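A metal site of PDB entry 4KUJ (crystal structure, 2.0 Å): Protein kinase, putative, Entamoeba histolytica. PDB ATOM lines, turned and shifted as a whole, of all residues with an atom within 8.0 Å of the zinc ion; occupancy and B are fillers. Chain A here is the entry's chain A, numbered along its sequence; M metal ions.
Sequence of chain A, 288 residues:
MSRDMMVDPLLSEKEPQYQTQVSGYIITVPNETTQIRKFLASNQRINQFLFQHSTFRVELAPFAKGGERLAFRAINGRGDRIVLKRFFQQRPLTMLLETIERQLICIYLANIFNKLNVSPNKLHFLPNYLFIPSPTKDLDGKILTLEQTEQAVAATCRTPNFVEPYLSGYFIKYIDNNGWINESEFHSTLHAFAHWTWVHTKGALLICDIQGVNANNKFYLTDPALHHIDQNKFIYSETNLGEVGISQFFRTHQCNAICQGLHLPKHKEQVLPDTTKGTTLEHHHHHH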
ATOM      1  N   SER A 188      15.014  15.338  -4.134  1.00  0.00           N
ATOM      2  CA  SER A 188      15.482  15.451  -2.780  1.00  0.00           C
ATOM      3  C   SER A 188      16.096  14.134  -2.304  1.00  0.00           C
ATOM      4  O   SER A 188      17.018  14.130  -1.489  1.00  0.00           O
ATOM      5  CB  SER A 188      14.321  15.871  -1.869  1.00  0.00           C
ATOM      6  OG  SER A 188      13.425  14.784  -1.706  1.00  0.00           O
ATOM      7  N   HIS A 191      19.869  14.175  -3.155  1.00  0.00           N
ATOM      8  CA  HIS A 191      20.633  15.088  -2.286  1.00  0.00           C
ATOM      9  C   HIS A 191      20.753  14.568  -0.893  1.00  0.00           C
ATOM     10  O   HIS A 191      21.800  14.676  -0.273  1.00  0.00           O
ATOM     11  CB  HIS A 191      20.026  16.494  -2.349  1.00  0.00           C
ATOM     12  CG  HIS A 191      20.292  17.183  -3.680  1.00  0.00           C
ATOM     13  ND1 HIS A 191      19.542  16.960  -4.783  1.00  0.00           N
ATOM     14  CD2 HIS A 191      21.295  18.041  -4.055  1.00  0.00           C
ATOM     15  CE1 HIS A 191      20.034  17.668  -5.806  1.00  0.00           C
ATOM     16  NE2 HIS A 191      21.100  18.349  -5.350  1.00  0.00           N
ATOM     17  N   ALA A 192      19.690  13.961  -0.375  1.00  0.00           N
ATOM     18  CA  ALA A 192      19.767  13.427   0.992  1.00  0.00           C
ATOM     19  C   ALA A 192      20.716  12.207   1.032  1.00  0.00           C
ATOM     20  O   ALA A 192      21.430  11.968   2.028  1.00  0.00           O
ATOM     21  CB  ALA A 192      18.373  13.047   1.484  1.00  0.00           C
ATOM     22  N   PHE A 193      20.708  11.441  -0.057  1.00  0.00           N
ATOM     23  CA  PHE A 193      21.633  10.305  -0.157  1.00  0.00           C
ATOM     24  C   PHE A 193      23.069  10.780  -0.024  1.00  0.00           C
ATOM     25  O   PHE A 193      23.854  10.204   0.748  1.00  0.00           O
ATOM     26  CB  PHE A 193      21.444   9.528  -1.457  1.00  0.00           C
ATOM     27  CG  PHE A 193      22.506   8.458  -1.679  1.00  0.00           C
ATOM     28  CD1 PHE A 193      22.497   7.289  -0.922  1.00  0.00           C
ATOM     29  CD2 PHE A 193      23.486   8.633  -2.614  1.00  0.00           C
ATOM     30  CE1 PHE A 193      23.478   6.330  -1.106  1.00  0.00           C
ATOM     31  CE2 PHE A 193      24.481   7.672  -2.812  1.00  0.00           C
ATOM     32  CZ  PHE A 193      24.465   6.521  -2.062  1.00  0.00           C
ATOM     33  N   ALA A 194      23.429  11.813  -0.798  1.00  0.00           N
ATOM     34  CA  ALA A 194      24.792  12.292  -0.789  1.00  0.00           C
ATOM     35  C   ALA A 194      25.186  12.747   0.634  1.00  0.00           C
ATOM     36  O   ALA A 194      26.202  12.336   1.170  1.00  0.00           O
ATOM     37  CB  ALA A 194      24.971  13.430  -1.798  1.00  0.00           C
ATOM     38  N   HIS A 195      24.364  13.590   1.239  1.00  0.00           N
ATOM     39  CA  HIS A 195      24.609  14.016   2.633  1.00  0.00           C
ATOM     40  C   HIS A 195      24.771  12.796   3.542  1.00  0.00           C
ATOM     41  O   HIS A 195      25.735  12.708   4.307  1.00  0.00           O
ATOM     42  CB  HIS A 195      23.438  14.887   3.099  1.00  0.00           C
ATOM     43  CG  HIS A 195      23.634  15.493   4.475  1.00  0.00           C
ATOM     44  ND1 HIS A 195      22.786  16.394   4.995  1.00  0.00           N
ATOM     45  CD2 HIS A 195      24.634  15.280   5.434  1.00  0.00           C
ATOM     46  CE1 HIS A 195      23.209  16.740   6.234  1.00  0.00           C
ATOM     47  NE2 HIS A 195      24.338  16.034   6.500  1.00  0.00           N
ATOM     48  N   TRP A 196      23.832  11.857   3.433  1.00  0.00           N
ATOM     49  CA  TRP A 196      23.837  10.637   4.249  1.00  0.00           C
ATOM     50  C   TRP A 196      25.115   9.832   4.085  1.00  0.00           C
ATOM     51  O   TRP A 196      25.645   9.288   5.068  1.00  0.00           O
ATOM     52  CB  TRP A 196      22.571   9.792   3.976  1.00  0.00           C
ATOM     53  CG  TRP A 196      22.598   8.468   4.711  1.00  0.00           C
ATOM     54  CD1 TRP A 196      22.190   8.194   6.013  1.00  0.00           C
ATOM     55  CD2 TRP A 196      23.124   7.213   4.203  1.00  0.00           C
ATOM     56  NE1 TRP A 196      22.412   6.870   6.326  1.00  0.00           N
ATOM     57  CE2 TRP A 196      22.987   6.230   5.280  1.00  0.00           C
ATOM     58  CE3 TRP A 196      23.689   6.820   2.992  1.00  0.00           C
ATOM     59  CZ2 TRP A 196      23.394   4.899   5.135  1.00  0.00           C
ATOM     60  CZ3 TRP A 196      24.103   5.493   2.852  1.00  0.00           C
ATOM     61  CH2 TRP A 196      23.955   4.557   3.888  1.00  0.00           C
ATOM     62  N   VAL A 199      27.471  11.115   6.385  1.00  0.00           N
ATOM     63  CA  VAL A 199      27.100  10.790   7.754  1.00  0.00           C
ATOM     64  C   VAL A 199      27.434   9.320   8.088  1.00  0.00           C
ATOM     65  O   VAL A 199      28.047   9.036   9.114  1.00  0.00           O
ATOM     66  CB  VAL A 199      25.622  11.041   8.033  1.00  0.00           C
ATOM     67  CG1 VAL A 199      25.299  10.597   9.457  1.00  0.00           C
ATOM     68  CG2 VAL A 199      25.311  12.531   7.844  1.00  0.00           C
ATOM     69  N   PHE A 249      30.291  20.458  -1.752  1.00  0.00           N
ATOM     70  CA  PHE A 249      28.946  19.908  -1.725  1.00  0.00           C
ATOM     71  C   PHE A 249      28.138  20.619  -0.642  1.00  0.00           C
ATOM     72  O   PHE A 249      27.015  21.072  -0.869  1.00  0.00           O
ATOM     73  CB  PHE A 249      28.934  18.376  -1.478  1.00  0.00           C
ATOM     74  CG  PHE A 249      27.537  17.843  -1.253  1.00  0.00           C
ATOM     75  CD1 PHE A 249      26.694  17.561  -2.341  1.00  0.00           C
ATOM     76  CD2 PHE A 249      27.033  17.732   0.029  1.00  0.00           C
ATOM     77  CE1 PHE A 249      25.387  17.142  -2.136  1.00  0.00           C
ATOM     78  CE2 PHE A 249      25.725  17.295   0.249  1.00  0.00           C
ATOM     79  CZ  PHE A 249      24.896  17.000  -0.827  1.00  0.00           C
ATOM     80  N   PHE A 250      28.723  20.730   0.548  1.00  0.00           N
ATOM     81  CA  PHE A 250      27.936  21.236   1.666  1.00  0.00           C
ATOM     82  C   PHE A 250      27.659  22.737   1.617  1.00  0.00           C
ATOM     83  O   PHE A 250      26.630  23.167   2.099  1.00  0.00           O
ATOM     84  CB  PHE A 250      28.537  20.803   3.009  1.00  0.00           C
ATOM     85  CG  PHE A 250      28.212  19.388   3.364  1.00  0.00           C
ATOM     86  CD1 PHE A 250      26.906  19.033   3.703  1.00  0.00           C
ATOM     87  CD2 PHE A 250      29.202  18.396   3.315  1.00  0.00           C
ATOM     88  CE1 PHE A 250      26.594  17.710   4.022  1.00  0.00           C
ATOM     89  CE2 PHE A 250      28.892  17.064   3.638  1.00  0.00           C
ATOM     90  CZ  PHE A 250      27.597  16.727   3.985  1.00  0.00           C
ATOM     91  N   HIS A 253      24.547  22.812  -0.235  1.00  0.00           N
ATOM     92  CA  HIS A 253      23.525  21.862   0.184  1.00  0.00           C
ATOM     93  C   HIS A 253      22.487  22.484   1.069  1.00  0.00           C
ATOM     94  O   HIS A 253      22.858  23.212   1.982  1.00  0.00           O
ATOM     95  CB  HIS A 253      24.163  20.679   0.919  1.00  0.00           C
ATOM     96  CG  HIS A 253      23.157  19.632   1.361  1.00  0.00           C
ATOM     97  ND1 HIS A 253      22.406  18.947   0.486  1.00  0.00           N
ATOM     98  CD2 HIS A 253      22.825  19.166   2.626  1.00  0.00           C
ATOM     99  CE1 HIS A 253      21.615  18.076   1.158  1.00  0.00           C
ATOM    100  NE2 HIS A 253      21.878  18.215   2.468  1.00  0.00           N
ATOM    101  N   GLN A 254      21.208  22.187   0.824  1.00  0.00           N
ATOM    102  CA  GLN A 254      20.131  22.507   1.752  1.00  0.00           C
ATOM    103  C   GLN A 254      19.539  21.204   2.218  1.00  0.00           C
ATOM    104  O   GLN A 254      19.123  20.400   1.380  1.00  0.00           O
ATOM    105  CB  GLN A 254      19.029  23.319   1.049  1.00  0.00           C
ATOM    106  CG  GLN A 254      19.518  24.681   0.535  1.00  0.00           C
ATOM    107  CD  GLN A 254      18.408  25.416  -0.183  1.00  0.00           C
ATOM    108  OE1 GLN A 254      18.225  25.250  -1.375  1.00  0.00           O
ATOM    109  NE2 GLN A 254      17.621  26.189   0.556  1.00  0.00           N
ATOM    110  N   CYS A 255      19.498  20.970   3.533  1.00  0.00           N
ATOM    111  CA  CYS A 255      18.911  19.757   4.024  1.00  0.00           C
ATOM    112  C   CYS A 255      17.447  19.813   3.659  1.00  0.00           C
ATOM    113  O   CYS A 255      16.807  20.854   3.786  1.00  0.00           O
ATOM    114  CB  CYS A 255      19.117  19.576   5.513  1.00  0.00           C
ATOM    115  SG  CYS A 255      20.755  18.883   5.858  1.00  0.00           S
ATOM    116  N   ASN A 256      16.959  18.692   3.135  1.00  0.00           N
ATOM    117  CA  ASN A 256      15.600  18.615   2.604  1.00  0.00           C
ATOM    118  C   ASN A 256      14.743  17.760   3.542  1.00  0.00           C
ATOM    119  O   ASN A 256      15.205  17.352   4.615  1.00  0.00           O
ATOM    120  CB  ASN A 256      15.589  18.135   1.158  1.00  0.00           C
ATOM    121  CG  ASN A 256      16.250  16.764   0.980  1.00  0.00           C
ATOM    122  OD1 ASN A 256      15.980  15.838   1.720  1.00  0.00           O
ATOM    123  ND2 ASN A 256      17.137  16.661  -0.006  1.00  0.00           N
ATOM    124  N   ALA A 257      13.499  17.505   3.174  1.00  0.00           N
ATOM    125  CA  ALA A 257      12.624  16.688   4.052  1.00  0.00           C
ATOM    126  C   ALA A 257      13.188  15.272   4.323  1.00  0.00           C
ATOM    127  O   ALA A 257      12.919  14.672   5.368  1.00  0.00           O
ATOM    128  CB  ALA A 257      11.199  16.603   3.500  1.00  0.00           C
ATOM    129  N   ILE A 258      13.961  14.748   3.371  1.00  0.00           N
ATOM    130  CA  ILE A 258      14.505  13.395   3.564  1.00  0.00           C
ATOM    131  C   ILE A 258      15.674  13.476   4.577  1.00  0.00           C
ATOM    132  O   ILE A 258      15.736  12.673   5.511  1.00  0.00           O
ATOM    133  CB  ILE A 258      14.930  12.712   2.228  1.00  0.00           C
ATOM    134  CG1 ILE A 258      13.775  12.653   1.199  1.00  0.00           C
ATOM    135  CG2 ILE A 258      15.518  11.313   2.493  1.00  0.00           C
ATOM    136  CD1 ILE A 258      12.402  12.221   1.742  1.00  0.00           C
ATOM    137  N   CYS A 259      16.554  14.470   4.420  1.00  0.00           N
ATOM    138  CA  CYS A 259      17.603  14.750   5.414  1.00  0.00           C
ATOM    139  C   CYS A 259      16.996  14.899   6.812  1.00  0.00           C
ATOM    140  O   CYS A 259      17.496  14.306   7.784  1.00  0.00           O
ATOM    141  CB  CYS A 259      18.349  16.051   5.065  1.00  0.00           C
ATOM    142  SG  CYS A 259      19.338  16.108   3.516  1.00  0.00           S
ATOM    143  N   GLN A 260      15.936  15.694   6.907  1.00  0.00           N
ATOM    144  CA  GLN A 260      15.276  15.982   8.190  1.00  0.00           C
ATOM    145  C   GLN A 260      14.727  14.713   8.818  1.00  0.00           C
ATOM    146  O   GLN A 260      14.933  14.474   9.995  1.00  0.00           O
ATOM    147  CB  GLN A 260      14.133  17.006   7.995  1.00  0.00           C
ATOM    148  CG  GLN A 260      14.591  18.432   7.669  1.00  0.00           C
ATOM    149  CD  GLN A 260      13.431  19.347   7.274  1.00  0.00           C
ATOM    150  OE1 GLN A 260      12.341  18.878   6.916  1.00  0.00           O
ATOM    151  NE2 GLN A 260      13.660  20.651   7.318  1.00  0.00           N
ATOM    152  N   LEU A 264      19.912  13.924   9.913  1.00  0.00           N
ATOM    153  CA  LEU A 264      21.324  13.988   9.546  1.00  0.00           C
ATOM    154  C   LEU A 264      22.005  15.200  10.189  1.00  0.00           C
ATOM    155  O   LEU A 264      21.572  16.358  10.007  1.00  0.00           O
ATOM    156  CB  LEU A 264      21.489  14.054   8.017  1.00  0.00           C
ATOM    157  CG  LEU A 264      20.846  12.947   7.181  1.00  0.00           C
ATOM    158  CD1 LEU A 264      21.165  13.187   5.701  1.00  0.00           C
ATOM    159  CD2 LEU A 264      21.373  11.568   7.634  1.00  0.00           C
ATOM    160  N   PRO A 265      23.098  14.962  10.893  1.00  0.00           N
ATOM    161  CA  PRO A 265      23.862  16.103  11.345  1.00  0.00           C
ATOM    162  C   PRO A 265      24.467  16.865  10.135  1.00  0.00           C
ATOM    163  O   PRO A 265      24.835  16.254   9.113  1.00  0.00           O
ATOM    164  CB  PRO A 265      24.964  15.487  12.199  1.00  0.00           C
ATOM    165  CG  PRO A 265      25.121  14.104  11.629  1.00  0.00           C
ATOM    166  CD  PRO A 265      23.748  13.688  11.193  1.00  0.00           C
ATOM    167  N   LYS A 266      24.537  18.188  10.276  1.00  0.00           N
ATOM    168  CA  LYS A 266      24.974  19.065   9.216  1.00  0.00           C
ATOM    169  C   LYS A 266      26.455  19.271   9.288  1.00  0.00           C
ATOM    170  O   LYS A 266      27.067  19.276  10.360  1.00  0.00           O
ATOM    171  CB  LYS A 266      24.254  20.394   9.341  1.00  0.00           C
ATOM    172  CG  LYS A 266      22.749  20.305   9.017  1.00  0.00           C
ATOM    173  CD  LYS A 266      22.066  21.649   9.259  1.00  0.00           C
ATOM    174  CE  LYS A 266      20.572  21.601   8.942  1.00  0.00           C
ATOM    175  NZ  LYS A 266      20.046  22.999   8.763  1.00  0.00           N
ATOM    176  N   HIS A 267      27.038  19.447   8.103  1.00  0.00           N
ATOM    177  CA  HIS A 267      28.424  19.775   7.966  1.00  0.00           C
ATOM    178  C   HIS A 267      28.589  21.217   8.380  1.00  0.00           C
ATOM    179  O   HIS A 267      27.739  22.070   8.076  1.00  0.00           O
ATOM    180  CB  HIS A 267      28.831  19.584   6.520  1.00  0.00           C
ATOM    181  CG  HIS A 267      30.329  19.653   6.289  1.00  0.00           C
ATOM    182  ND1 HIS A 267      30.988  20.828   6.239  1.00  0.00           N
ATOM    183  CD2 HIS A 267      31.258  18.669   6.031  1.00  0.00           C
ATOM    184  CE1 HIS A 267      32.295  20.593   6.004  1.00  0.00           C
ATOM    185  NE2 HIS A 267      32.461  19.261   5.893  1.00  0.00           N
ATOM    186  N   GLN A 270      27.795  24.041   6.061  1.00  0.00           N
ATOM    187  CA  GLN A 270      26.433  24.332   5.635  1.00  0.00           C
ATOM    188  C   GLN A 270      25.991  25.656   6.216  1.00  0.00           C
ATOM    189  O   GLN A 270      26.177  25.934   7.402  1.00  0.00           O
ATOM    190  CB  GLN A 270      25.453  23.276   6.089  1.00  0.00           C
ATOM    191  CG  GLN A 270      25.377  22.082   5.174  1.00  0.00           C
ATOM    192  CD  GLN A 270      24.333  21.095   5.630  1.00  0.00           C
ATOM    193  OE1 GLN A 270      24.653  19.971   6.048  1.00  0.00           O
ATOM    194  NE2 GLN A 270      23.071  21.482   5.525  1.00  0.00           N
ATOM    195  N   ASP A 274      17.171  25.034   5.397  1.00  0.00           N
ATOM    196  CA  ASP A 274      16.511  23.808   4.927  1.00  0.00           C
ATOM    197  C   ASP A 274      15.512  24.148   3.834  1.00  0.00           C
ATOM    198  O   ASP A 274      15.041  25.273   3.771  1.00  0.00           O
ATOM    199  CB  ASP A 274      15.757  23.117   6.046  1.00  0.00           C
ATOM    200  CG  ASP A 274      16.658  22.499   7.095  1.00  0.00           C
ATOM    201  OD1 ASP A 274      17.899  22.565   7.021  1.00  0.00           O
ATOM    202  OD2 ASP A 274      16.071  21.934   8.046  1.00  0.00           O
HETATM  203 ZN    ZN M   1      21.113  17.309   4.159  1.00  0.00          ZN
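A ring nitrogen (NE2) of His 195 lies within hydrogen-bond range of the backbone carbonyl oxygen (O) of Pro 265, 2.7 Å away. The backbone carbonyl oxygen (O) of Cys 259 is in hydrogen-bond range of the backbone NH (N) of Leu 264, 3.2 Å away. The side-chain amide oxygen of Asn 256 is in hydrogen-bond range of the backbone NH of Cys 259 (3.1 Å). SG of Cys 255 sits close to NE2 of Gln 270 (3.5 Å).
Of the 24 residues printed, 4 come within 4 Å of the zinc ion. The nearest printed residue that does not touch the zinc ion is Leu 264 (4.4 Å).
The zinc ion is bound by NE2 of His 253 (2.1 Å), ND1 of His 195 (2.1 Å), SG of Cys 259 (2.2 Å) and SG of Cys 255 (2.3 Å).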
